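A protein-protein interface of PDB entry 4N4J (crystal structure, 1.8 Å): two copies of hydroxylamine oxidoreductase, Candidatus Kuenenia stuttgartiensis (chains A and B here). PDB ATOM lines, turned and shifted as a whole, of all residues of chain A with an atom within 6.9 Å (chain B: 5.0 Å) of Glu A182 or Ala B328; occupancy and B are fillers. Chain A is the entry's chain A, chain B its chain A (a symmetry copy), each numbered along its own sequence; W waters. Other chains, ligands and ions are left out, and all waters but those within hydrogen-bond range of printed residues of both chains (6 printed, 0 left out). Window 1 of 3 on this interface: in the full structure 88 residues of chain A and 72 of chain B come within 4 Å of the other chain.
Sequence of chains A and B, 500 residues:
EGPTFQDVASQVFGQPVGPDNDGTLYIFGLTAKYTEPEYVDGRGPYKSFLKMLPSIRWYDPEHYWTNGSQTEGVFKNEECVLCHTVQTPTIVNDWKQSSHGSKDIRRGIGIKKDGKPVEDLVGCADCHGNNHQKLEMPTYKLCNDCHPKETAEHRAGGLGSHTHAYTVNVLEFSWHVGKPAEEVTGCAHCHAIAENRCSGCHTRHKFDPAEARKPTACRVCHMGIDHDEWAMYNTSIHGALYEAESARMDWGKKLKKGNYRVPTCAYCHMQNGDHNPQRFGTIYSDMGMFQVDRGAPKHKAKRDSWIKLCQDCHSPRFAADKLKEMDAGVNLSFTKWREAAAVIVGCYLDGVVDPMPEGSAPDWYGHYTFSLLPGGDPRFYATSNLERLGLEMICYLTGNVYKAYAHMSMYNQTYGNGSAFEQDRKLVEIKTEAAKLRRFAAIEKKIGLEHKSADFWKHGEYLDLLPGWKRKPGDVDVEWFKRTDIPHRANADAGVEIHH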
ATOM      1  N   ASP A  20      20.380 -33.236 -14.625  1.00  0.00           N
ATOM      2  CA  ASP A  20      20.011 -32.183 -13.679  1.00  0.00           C
ATOM      3  C   ASP A  20      18.936 -32.625 -12.684  1.00  0.00           C
ATOM      4  O   ASP A  20      18.895 -32.136 -11.557  1.00  0.00           O
ATOM      5  CB  ASP A  20      19.564 -30.909 -14.416  1.00  0.00           C
ATOM      6  CG  ASP A  20      18.438 -31.151 -15.419  1.00  0.00           C
ATOM      7  OD1 ASP A  20      18.137 -30.217 -16.191  1.00  0.00           O
ATOM      8  OD2 ASP A  20      17.854 -32.256 -15.451  1.00  0.00           O
ATOM      9  N   TYR A  34      21.079 -30.933 -18.987  1.00  0.00           N
ATOM     10  CA  TYR A  34      19.694 -30.495 -19.073  1.00  0.00           C
ATOM     11  C   TYR A  34      18.808 -31.659 -19.485  1.00  0.00           C
ATOM     12  O   TYR A  34      19.130 -32.398 -20.419  1.00  0.00           O
ATOM     13  CB  TYR A  34      19.539 -29.341 -20.059  1.00  0.00           C
ATOM     14  CG  TYR A  34      18.099 -28.988 -20.372  1.00  0.00           C
ATOM     15  CD1 TYR A  34      17.348 -28.195 -19.505  1.00  0.00           C
ATOM     16  CD2 TYR A  34      17.494 -29.438 -21.541  1.00  0.00           C
ATOM     17  CE1 TYR A  34      16.026 -27.865 -19.796  1.00  0.00           C
ATOM     18  CE2 TYR A  34      16.184 -29.114 -21.842  1.00  0.00           C
ATOM     19  CZ  TYR A  34      15.452 -28.329 -20.968  1.00  0.00           C
ATOM     20  OH  TYR A  34      14.150 -28.017 -21.282  1.00  0.00           O
ATOM     21  N   THR A  35      17.704 -31.825 -18.767  1.00  0.00           N
ATOM     22  CA  THR A  35      16.691 -32.801 -19.127  1.00  0.00           C
ATOM     23  C   THR A  35      15.392 -32.050 -19.356  1.00  0.00           C
ATOM     24  O   THR A  35      15.002 -31.194 -18.565  1.00  0.00           O
ATOM     25  CB  THR A  35      16.488 -33.858 -18.033  1.00  0.00           C
ATOM     26  OG1 THR A  35      15.923 -33.245 -16.870  1.00  0.00           O
ATOM     27  CG2 THR A  35      17.815 -34.519 -17.672  1.00  0.00           C
ATOM     28  N   GLU A  36      14.736 -32.369 -20.457  1.00  0.00           N
ATOM     29  CA  GLU A  36      13.480 -31.742 -20.800  1.00  0.00           C
ATOM     30  C   GLU A  36      12.432 -32.183 -19.781  1.00  0.00           C
ATOM     31  O   GLU A  36      12.292 -33.375 -19.520  1.00  0.00           O
ATOM     32  CB  GLU A  36      13.091 -32.177 -22.212  1.00  0.00           C
ATOM     33  CG  GLU A  36      12.147 -31.274 -22.915  1.00  0.00           C
ATOM     34  CD  GLU A  36      11.840 -31.775 -24.304  1.00  0.00           C
ATOM     35  OE1 GLU A  36      12.504 -31.323 -25.255  1.00  0.00           O
ATOM     36  OE2 GLU A  36      10.957 -32.641 -24.435  1.00  0.00           O
ATOM     37  N   PRO A  37      11.713 -31.225 -19.169  1.00  0.00           N
ATOM     38  CA  PRO A  37      10.636 -31.624 -18.267  1.00  0.00           C
ATOM     39  C   PRO A  37       9.481 -32.251 -19.037  1.00  0.00           C
ATOM     40  O   PRO A  37       9.388 -32.074 -20.255  1.00  0.00           O
ATOM     41  CB  PRO A  37      10.191 -30.309 -17.614  1.00  0.00           C
ATOM     42  CG  PRO A  37      10.785 -29.229 -18.396  1.00  0.00           C
ATOM     43  CD  PRO A  37      11.838 -29.763 -19.293  1.00  0.00           C
ATOM     44  N   TYR A  39       6.073 -32.354 -20.601  1.00  0.00           N
ATOM     45  CA  TYR A  39       5.223 -31.302 -21.139  1.00  0.00           C
ATOM     46  C   TYR A  39       3.856 -31.842 -21.494  1.00  0.00           C
ATOM     47  O   TYR A  39       3.670 -33.052 -21.638  1.00  0.00           O
ATOM     48  CB  TYR A  39       5.815 -30.742 -22.426  1.00  0.00           C
ATOM     49  CG  TYR A  39       7.124 -29.999 -22.306  1.00  0.00           C
ATOM     50  CD1 TYR A  39       7.338 -29.043 -21.316  1.00  0.00           C
ATOM     51  CD2 TYR A  39       8.138 -30.220 -23.227  1.00  0.00           C
ATOM     52  CE1 TYR A  39       8.550 -28.345 -21.243  1.00  0.00           C
ATOM     53  CE2 TYR A  39       9.333 -29.539 -23.161  1.00  0.00           C
ATOM     54  CZ  TYR A  39       9.541 -28.602 -22.171  1.00  0.00           C
ATOM     55  OH  TYR A  39      10.747 -27.937 -22.145  1.00  0.00           O
ATOM     56  N   LYS A  51       4.602 -26.030 -26.167  1.00  0.00           N
ATOM     57  CA  LYS A  51       4.411 -26.891 -25.024  1.00  0.00           C
ATOM     58  C   LYS A  51       4.000 -26.062 -23.816  1.00  0.00           C
ATOM     59  O   LYS A  51       4.145 -24.834 -23.799  1.00  0.00           O
ATOM     60  CB  LYS A  51       5.703 -27.640 -24.693  1.00  0.00           C
ATOM     61  CG  LYS A  51       6.306 -28.426 -25.845  1.00  0.00           C
ATOM     62  CD  LYS A  51       5.397 -29.551 -26.311  1.00  0.00           C
ATOM     63  CE  LYS A  51       6.037 -30.332 -27.459  1.00  0.00           C
ATOM     64  NZ  LYS A  51       5.014 -31.009 -28.308  1.00  0.00           N
ATOM     65  N   MET A  52       3.481 -26.759 -22.814  1.00  0.00           N
ATOM     66  CA  MET A  52       3.209 -26.194 -21.500  1.00  0.00           C
ATOM     67  C   MET A  52       3.652 -27.206 -20.471  1.00  0.00           C
ATOM     68  O   MET A  52       3.654 -28.406 -20.748  1.00  0.00           O
ATOM     69  CB  MET A  52       1.711 -25.966 -21.317  1.00  0.00           C
ATOM     70  CG  MET A  52       1.128 -24.891 -22.200  1.00  0.00           C
ATOM     71  SD  MET A  52       1.545 -23.241 -21.611  1.00  0.00           S
ATOM     72  CE  MET A  52       1.063 -22.276 -23.040  1.00  0.00           C
ATOM     73  N   LEU A  53       4.008 -26.740 -19.277  1.00  0.00           N
ATOM     74  CA  LEU A  53       4.144 -27.651 -18.155  1.00  0.00           C
ATOM     75  C   LEU A  53       2.736 -28.123 -17.783  1.00  0.00           C
ATOM     76  O   LEU A  53       1.765 -27.392 -17.996  1.00  0.00           O
ATOM     77  CB  LEU A  53       4.826 -26.981 -16.963  1.00  0.00           C
ATOM     78  CG  LEU A  53       6.320 -26.685 -17.116  1.00  0.00           C
ATOM     79  CD1 LEU A  53       6.848 -26.089 -15.824  1.00  0.00           C
ATOM     80  CD2 LEU A  53       7.115 -27.934 -17.494  1.00  0.00           C
ATOM     81  N   LYS A 179      10.308 -19.706 -26.718  1.00  0.00           N
ATOM     82  CA  LYS A 179      11.114 -20.187 -25.599  1.00  0.00           C
ATOM     83  C   LYS A 179      10.630 -21.527 -25.048  1.00  0.00           C
ATOM     84  O   LYS A 179       9.452 -21.864 -25.174  1.00  0.00           O
ATOM     85  CB  LYS A 179      11.118 -19.140 -24.481  1.00  0.00           C
ATOM     86  CG  LYS A 179      11.922 -17.901 -24.821  1.00  0.00           C
ATOM     87  CD  LYS A 179      11.812 -16.834 -23.735  1.00  0.00           C
ATOM     88  CE  LYS A 179      12.895 -15.785 -23.886  1.00  0.00           C
ATOM     89  NZ  LYS A 179      14.237 -16.320 -23.508  1.00  0.00           N
ATOM     90  N   PRO A 180      11.540 -22.297 -24.418  1.00  0.00           N
ATOM     91  CA  PRO A 180      11.117 -23.521 -23.746  1.00  0.00           C
ATOM     92  C   PRO A 180      10.036 -23.235 -22.709  1.00  0.00           C
ATOM     93  O   PRO A 180      10.117 -22.240 -21.995  1.00  0.00           O
ATOM     94  CB  PRO A 180      12.398 -24.014 -23.066  1.00  0.00           C
ATOM     95  CG  PRO A 180      13.488 -23.425 -23.849  1.00  0.00           C
ATOM     96  CD  PRO A 180      12.993 -22.088 -24.304  1.00  0.00           C
ATOM     97  N   ALA A 181       9.045 -24.114 -22.624  1.00  0.00           N
ATOM     98  CA  ALA A 181       7.839 -23.838 -21.844  1.00  0.00           C
ATOM     99  C   ALA A 181       8.124 -23.504 -20.385  1.00  0.00           C
ATOM    100  O   ALA A 181       7.530 -22.578 -19.833  1.00  0.00           O
ATOM    101  CB  ALA A 181       6.870 -25.009 -21.936  1.00  0.00           C
ATOM    102  N   GLU A 182       9.041 -24.242 -19.764  1.00  0.00           N
ATOM    103  CA  GLU A 182       9.334 -24.039 -18.345  1.00  0.00           C
ATOM    104  C   GLU A 182       9.998 -22.697 -18.050  1.00  0.00           C
ATOM    105  O   GLU A 182      10.002 -22.247 -16.905  1.00  0.00           O
ATOM    106  CB  GLU A 182      10.179 -25.185 -17.775  1.00  0.00           C
ATOM    107  CG  GLU A 182      11.617 -25.223 -18.252  1.00  0.00           C
ATOM    108  CD  GLU A 182      11.835 -26.119 -19.452  1.00  0.00           C
ATOM    109  OE1 GLU A 182      12.909 -26.750 -19.500  1.00  0.00           O
ATOM    110  OE2 GLU A 182      10.952 -26.192 -20.344  1.00  0.00           O
ATOM    111  N   GLU A 183      10.561 -22.060 -19.070  1.00  0.00           N
ATOM    112  CA  GLU A 183      11.129 -20.727 -18.911  1.00  0.00           C
ATOM    113  C   GLU A 183      10.055 -19.651 -18.726  1.00  0.00           C
ATOM    114  O   GLU A 183      10.291 -18.633 -18.075  1.00  0.00           O
ATOM    115  CB  GLU A 183      11.978 -20.378 -20.131  1.00  0.00           C
ATOM    116  CG  GLU A 183      12.783 -19.113 -19.957  1.00  0.00           C
ATOM    117  CD  GLU A 183      13.590 -18.760 -21.169  1.00  0.00           C
ATOM    118  OE1 GLU A 183      14.152 -17.646 -21.181  1.00  0.00           O
ATOM    119  OE2 GLU A 183      13.660 -19.586 -22.108  1.00  0.00           O
ATOM    120  N   VAL A 184       8.879 -19.888 -19.297  1.00  0.00           N
ATOM    121  CA  VAL A 184       7.860 -18.855 -19.419  1.00  0.00           C
ATOM    122  C   VAL A 184       6.523 -19.242 -18.788  1.00  0.00           C
ATOM    123  O   VAL A 184       5.499 -18.631 -19.071  1.00  0.00           O
ATOM    124  CB  VAL A 184       7.676 -18.461 -20.889  1.00  0.00           C
ATOM    125  CG1 VAL A 184       8.931 -17.759 -21.386  1.00  0.00           C
ATOM    126  CG2 VAL A 184       7.356 -19.689 -21.755  1.00  0.00           C
ATOM    127  N   THR A 185       6.551 -20.237 -17.909  1.00  0.00           N
ATOM    128  CA  THR A 185       5.374 -20.647 -17.142  1.00  0.00           C
ATOM    129  C   THR A 185       4.637 -19.461 -16.518  1.00  0.00           C
ATOM    130  O   THR A 185       3.418 -19.346 -16.645  1.00  0.00           O
ATOM    131  CB  THR A 185       5.782 -21.632 -16.034  1.00  0.00           C
ATOM    132  OG1 THR A 185       6.391 -22.781 -16.642  1.00  0.00           O
ATOM    133  CG2 THR A 185       4.581 -22.067 -15.215  1.00  0.00           C
ATOM    134  N   GLY A 186       5.388 -18.576 -15.870  1.00  0.00           N
ATOM    135  CA  GLY A 186       4.827 -17.388 -15.223  1.00  0.00           C
ATOM    136  C   GLY A 186       4.129 -16.439 -16.183  1.00  0.00           C
ATOM    137  O   GLY A 186       3.220 -15.714 -15.792  1.00  0.00           O
ATOM    138  N   LEU A 465      18.127 -25.206 -27.722  1.00  0.00           N
ATOM    139  CA  LEU A 465      16.774 -25.606 -27.328  1.00  0.00           C
ATOM    140  C   LEU A 465      15.680 -24.814 -28.046  1.00  0.00           C
ATOM    141  O   LEU A 465      14.505 -25.176 -27.975  1.00  0.00           O
ATOM    142  CB  LEU A 465      16.584 -25.426 -25.819  1.00  0.00           C
ATOM    143  CG  LEU A 465      17.552 -26.155 -24.889  1.00  0.00           C
ATOM    144  CD1 LEU A 465      17.318 -25.736 -23.441  1.00  0.00           C
ATOM    145  CD2 LEU A 465      17.421 -27.664 -25.033  1.00  0.00           C
ATOM    146  N   LYS B 324       7.120 -28.083  -8.599  1.00  0.00           N
ATOM    147  CA  LYS B 324       7.645 -28.654  -9.848  1.00  0.00           C
ATOM    148  C   LYS B 324       7.979 -27.570 -10.873  1.00  0.00           C
ATOM    149  O   LYS B 324       8.951 -27.696 -11.616  1.00  0.00           O
ATOM    150  CB  LYS B 324       6.673 -29.664 -10.464  1.00  0.00           C
ATOM    151  CG  LYS B 324       6.610 -31.008  -9.756  1.00  0.00           C
ATOM    152  CD  LYS B 324       5.444 -31.823 -10.310  1.00  0.00           C
ATOM    153  CE  LYS B 324       5.277 -33.166  -9.638  1.00  0.00           C
ATOM    154  NZ  LYS B 324       3.977 -33.790 -10.071  1.00  0.00           N
ATOM    155  N   GLU B 325       7.181 -26.505 -10.919  1.00  0.00           N
ATOM    156  CA  GLU B 325       7.491 -25.374 -11.791  1.00  0.00           C
ATOM    157  C   GLU B 325       8.836 -24.767 -11.423  1.00  0.00           C
ATOM    158  O   GLU B 325       9.620 -24.398 -12.298  1.00  0.00           O
ATOM    159  CB  GLU B 325       6.403 -24.309 -11.719  1.00  0.00           C
ATOM    160  CG  GLU B 325       5.123 -24.724 -12.392  1.00  0.00           C
ATOM    161  CD  GLU B 325       3.977 -23.783 -12.085  1.00  0.00           C
ATOM    162  OE1 GLU B 325       4.227 -22.656 -11.599  1.00  0.00           O
ATOM    163  OE2 GLU B 325       2.823 -24.177 -12.340  1.00  0.00           O
ATOM    164  N   MET B 326       9.093 -24.672 -10.123  1.00  0.00           N
ATOM    165  CA  MET B 326      10.379 -24.220  -9.622  1.00  0.00           C
ATOM    166  C   MET B 326      11.500 -25.119 -10.120  1.00  0.00           C
ATOM    167  O   MET B 326      12.487 -24.635 -10.673  1.00  0.00           O
ATOM    168  CB  MET B 326      10.381 -24.198  -8.094  1.00  0.00           C
ATOM    169  CG  MET B 326      11.732 -23.865  -7.477  1.00  0.00           C
ATOM    170  SD  MET B 326      11.695 -23.832  -5.683  1.00  0.00           S
ATOM    171  CE  MET B 326      11.329 -25.555  -5.296  1.00  0.00           C
ATOM    172  N   ASP B 327      11.341 -26.424  -9.916  1.00  0.00           N
ATOM    173  CA  ASP B 327      12.361 -27.383 -10.328  1.00  0.00           C
ATOM    174  C   ASP B 327      12.682 -27.197 -11.809  1.00  0.00           C
ATOM    175  O   ASP B 327      13.849 -27.105 -12.195  1.00  0.00           O
ATOM    176  CB  ASP B 327      11.911 -28.825 -10.098  1.00  0.00           C
ATOM    177  CG  ASP B 327      11.543 -29.115  -8.663  1.00  0.00           C
ATOM    178  OD1 ASP B 327      12.106 -28.489  -7.734  1.00  0.00           O
ATOM    179  OD2 ASP B 327      10.679 -29.996  -8.465  1.00  0.00           O
ATOM    180  N   ALA B 328      11.635 -27.138 -12.633  1.00  0.00           N
ATOM    181  CA  ALA B 328      11.804 -27.006 -14.079  1.00  0.00           C
ATOM    182  C   ALA B 328      12.432 -25.671 -14.470  1.00  0.00           C
ATOM    183  O   ALA B 328      13.335 -25.619 -15.299  1.00  0.00           O
ATOM    184  CB  ALA B 328      10.461 -27.190 -14.785  1.00  0.00           C
ATOM    185  N   GLY B 329      11.956 -24.589 -13.866  1.00  0.00           N
ATOM    186  CA  GLY B 329      12.487 -23.262 -14.151  1.00  0.00           C
ATOM    187  C   GLY B 329      13.947 -23.134 -13.772  1.00  0.00           C
ATOM    188  O   GLY B 329      14.735 -22.515 -14.492  1.00  0.00           O
ATOM    189  N   VAL B 330      14.302 -23.715 -12.631  1.00  0.00           N
ATOM    190  CA  VAL B 330      15.681 -23.726 -12.167  1.00  0.00           C
ATOM    191  C   VAL B 330      16.574 -24.500 -13.130  1.00  0.00           C
ATOM    192  O   VAL B 330      17.636 -24.014 -13.518  1.00  0.00           O
ATOM    193  CB  VAL B 330      15.790 -24.299 -10.738  1.00  0.00           C
ATOM    194  CG1 VAL B 330      17.244 -24.638 -10.392  1.00  0.00           C
ATOM    195  CG2 VAL B 330      15.221 -23.300  -9.746  1.00  0.00           C
ATOM    196  N   ASN B 331      16.135 -25.684 -13.543  1.00  0.00           N
ATOM    197  CA  ASN B 331      16.937 -26.489 -14.469  1.00  0.00           C
ATOM    198  C   ASN B 331      17.165 -25.797 -15.804  1.00  0.00           C
ATOM    199  O   ASN B 331      18.259 -25.858 -16.355  1.00  0.00           O
ATOM    200  CB  ASN B 331      16.323 -27.872 -14.672  1.00  0.00           C
ATOM    201  CG  ASN B 331      16.459 -28.750 -13.447  1.00  0.00           C
ATOM    202  OD1 ASN B 331      17.258 -28.468 -12.553  1.00  0.00           O
ATOM    203  ND2 ASN B 331      15.686 -29.828 -13.403  1.00  0.00           N
ATOM    204  N   LEU B 332      16.143 -25.124 -16.319  1.00  0.00           N
ATOM    205  CA  LEU B 332      16.303 -24.362 -17.551  1.00  0.00           C
ATOM    206  C   LEU B 332      17.303 -23.221 -17.352  1.00  0.00           C
ATOM    207  O   LEU B 332      18.162 -22.982 -18.208  1.00  0.00           O
ATOM    208  CB  LEU B 332      14.944 -23.835 -18.027  1.00  0.00           C
ATOM    209  CG  LEU B 332      14.849 -23.188 -19.411  1.00  0.00           C
ATOM    210  CD1 LEU B 332      15.388 -21.768 -19.391  1.00  0.00           C
ATOM    211  CD2 LEU B 332      15.558 -24.022 -20.475  1.00  0.00           C
ATOM    212  N   TYR B 405      11.057 -18.429  -8.255  1.00  0.00           N
ATOM    213  CA  TYR B 405      10.156 -19.571  -8.317  1.00  0.00           C
ATOM    214  C   TYR B 405       9.710 -20.021  -6.936  1.00  0.00           C
ATOM    215  O   TYR B 405       8.536 -20.333  -6.729  1.00  0.00           O
ATOM    216  CB  TYR B 405      10.812 -20.730  -9.061  1.00  0.00           C
ATOM    217  CG  TYR B 405      10.648 -20.628 -10.552  1.00  0.00           C
ATOM    218  CD1 TYR B 405      11.686 -20.186 -11.358  1.00  0.00           C
ATOM    219  CD2 TYR B 405       9.446 -20.966 -11.155  1.00  0.00           C
ATOM    220  CE1 TYR B 405      11.533 -20.089 -12.726  1.00  0.00           C
ATOM    221  CE2 TYR B 405       9.278 -20.869 -12.524  1.00  0.00           C
ATOM    222  CZ  TYR B 405      10.327 -20.431 -13.305  1.00  0.00           C
ATOM    223  OH  TYR B 405      10.181 -20.337 -14.666  1.00  0.00           O
HETATM  224  O   HOH W   1       7.956 -18.647 -14.958  1.00  0.00           O
HETATM  225  O   HOH W   2      11.850 -18.671 -15.869  1.00  0.00           O
HETATM  226  O   HOH W   3       8.598 -23.345 -14.926  1.00  0.00           O
HETATM  227  O   HOH W   4      13.758 -27.684 -17.004  1.00  0.00           O
HETATM  228  O   HOH W   5      13.943 -30.112 -15.838  1.00  0.00           O
HETATM  229  O   HOH W   6      19.797 -28.053 -16.347  1.00  0.00           O
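The side-chain carboxylate (OD2) of Asp A20 is in hydrogen-bond range of the side-chain hydroxyl (OG1) of Thr A35 (2.6 Å).
OH of Tyr A34 lies within hydrogen-bond range of OE1 of Glu A182, at 2.5 Å.
The side-chain hydroxyl (OH) of Tyr A39 sits at hydrogen-bond distance from the side-chain carboxylate (OE2) of Glu A182 (2.5 Å).
The side-chain amino group (NZ) of Lys A179 is in salt-bridge range of the side-chain carboxylate (OE1) of Glu A183 (2.7 Å).
The side-chain hydroxyl (OG1) of Thr A185 is in hydrogen-bond range of the backbone carbonyl oxygen (O) of Ala A181 (3.4 Å).
O of Asp B327 lies close to ND2 of Asn B331, 3.5 Å away.
Printed residues of chain B within 4 Å of Asp A20: Asn B331.
Of chain B, only Ala B328 (3.4 Å), Gly B329 (3.8 Å), Leu B332 (3.6 Å) and Tyr B405 (2.9 Å) come within 4 Å of Glu A182.
Printed residues of chain B within 4 Å of Leu A465: Leu B332.
Of chain A, only Leu A53 and Glu A182 come within 4 Å of Ala B328.
Printed residues of chain A within 4 Å of Gly B329: Glu A182 (3.8 Å).
Water W2 bridges the side-chain hydroxyl (OH) of Tyr B405 (2.6 Å) and the backbone carbonyl oxygen (O) of Glu A183 (2.7 Å).
Water W3 lies within hydrogen-bond range of O of Glu A182 (2.7 Å), OG1 of Thr A185 (2.9 Å), O of Glu B325 (3.0 Å) and OH of Tyr B405 (3.4 Å).
Water W6 lies within hydrogen-bond range of O of Asn B331 (2.7 Å) and OD1 of Asp A20 (2.7 Å).
Water W4 bridges the backbone carbonyl oxygen (O) of Ala B328 (2.7 Å) and the side-chain carboxylate (OE1) of Glu A182 (2.8 Å).
Water W1 lies within hydrogen-bond range of the backbone NH (N) of Gly A186 (2.7 Å) and the side-chain hydroxyl (OH) of Tyr B405 (2.8 Å).
Water W5 lies within hydrogen-bond range of the side-chain amide nitrogen of Asn B331 (3.0 Å) and the backbone carbonyl oxygen of Thr A35 (3.1 Å).
No position is printed for both chains.
Of the 11 pairs that touch across the chains among the printed residues, none has its exchanged pair printed and touching as well.
Hydrophobic or aromatic side chains of chain A within 4 Å of the printed part of chain B: Tyr A34, Leu A53 and Leu A465.
Printed residues of chain B that touch a printed residue of chain A: Glu B325, Ala B328, Gly B329, Asn B331, Leu B332 and Tyr B405.
Hydrophobic or aromatic side chains of chain B that line the printed part of chain A: Ala B328, Leu B332 and Tyr B405.
Among the printed residues, no Asp or Glu carboxylate lies within 4 Å of a Lys or Arg side-chain nitrogen of the other chain.
Asp A20 touches Asn B331.
Tyr A34 touches Leu B332 (CE1 to CD2, 3.9 Å).
Leu A53 touches Ala B328.
Ala B328 touches Glu A182 (O to CG, 3.4 Å).
Glu A182 touches Gly B329 (O to CA, 3.8 Å).
CB of Leu B332 touches CG of Glu A182 (3.6 Å).
Leu B332 touches Glu A183 (CD1 to CB, 3.8 Å).
Tyr B405 touches Glu A183.
CD of Glu B325 touches CG2 of Thr A185 (3.6 Å).
CD1 of Leu A465 touches CD2 of Leu B332 (3.9 Å).
The backbone carbonyl oxygen (O) of Glu A182 sits at hydrogen-bond distance from the side-chain hydroxyl (OH) of Tyr B405 (2.9 Å).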
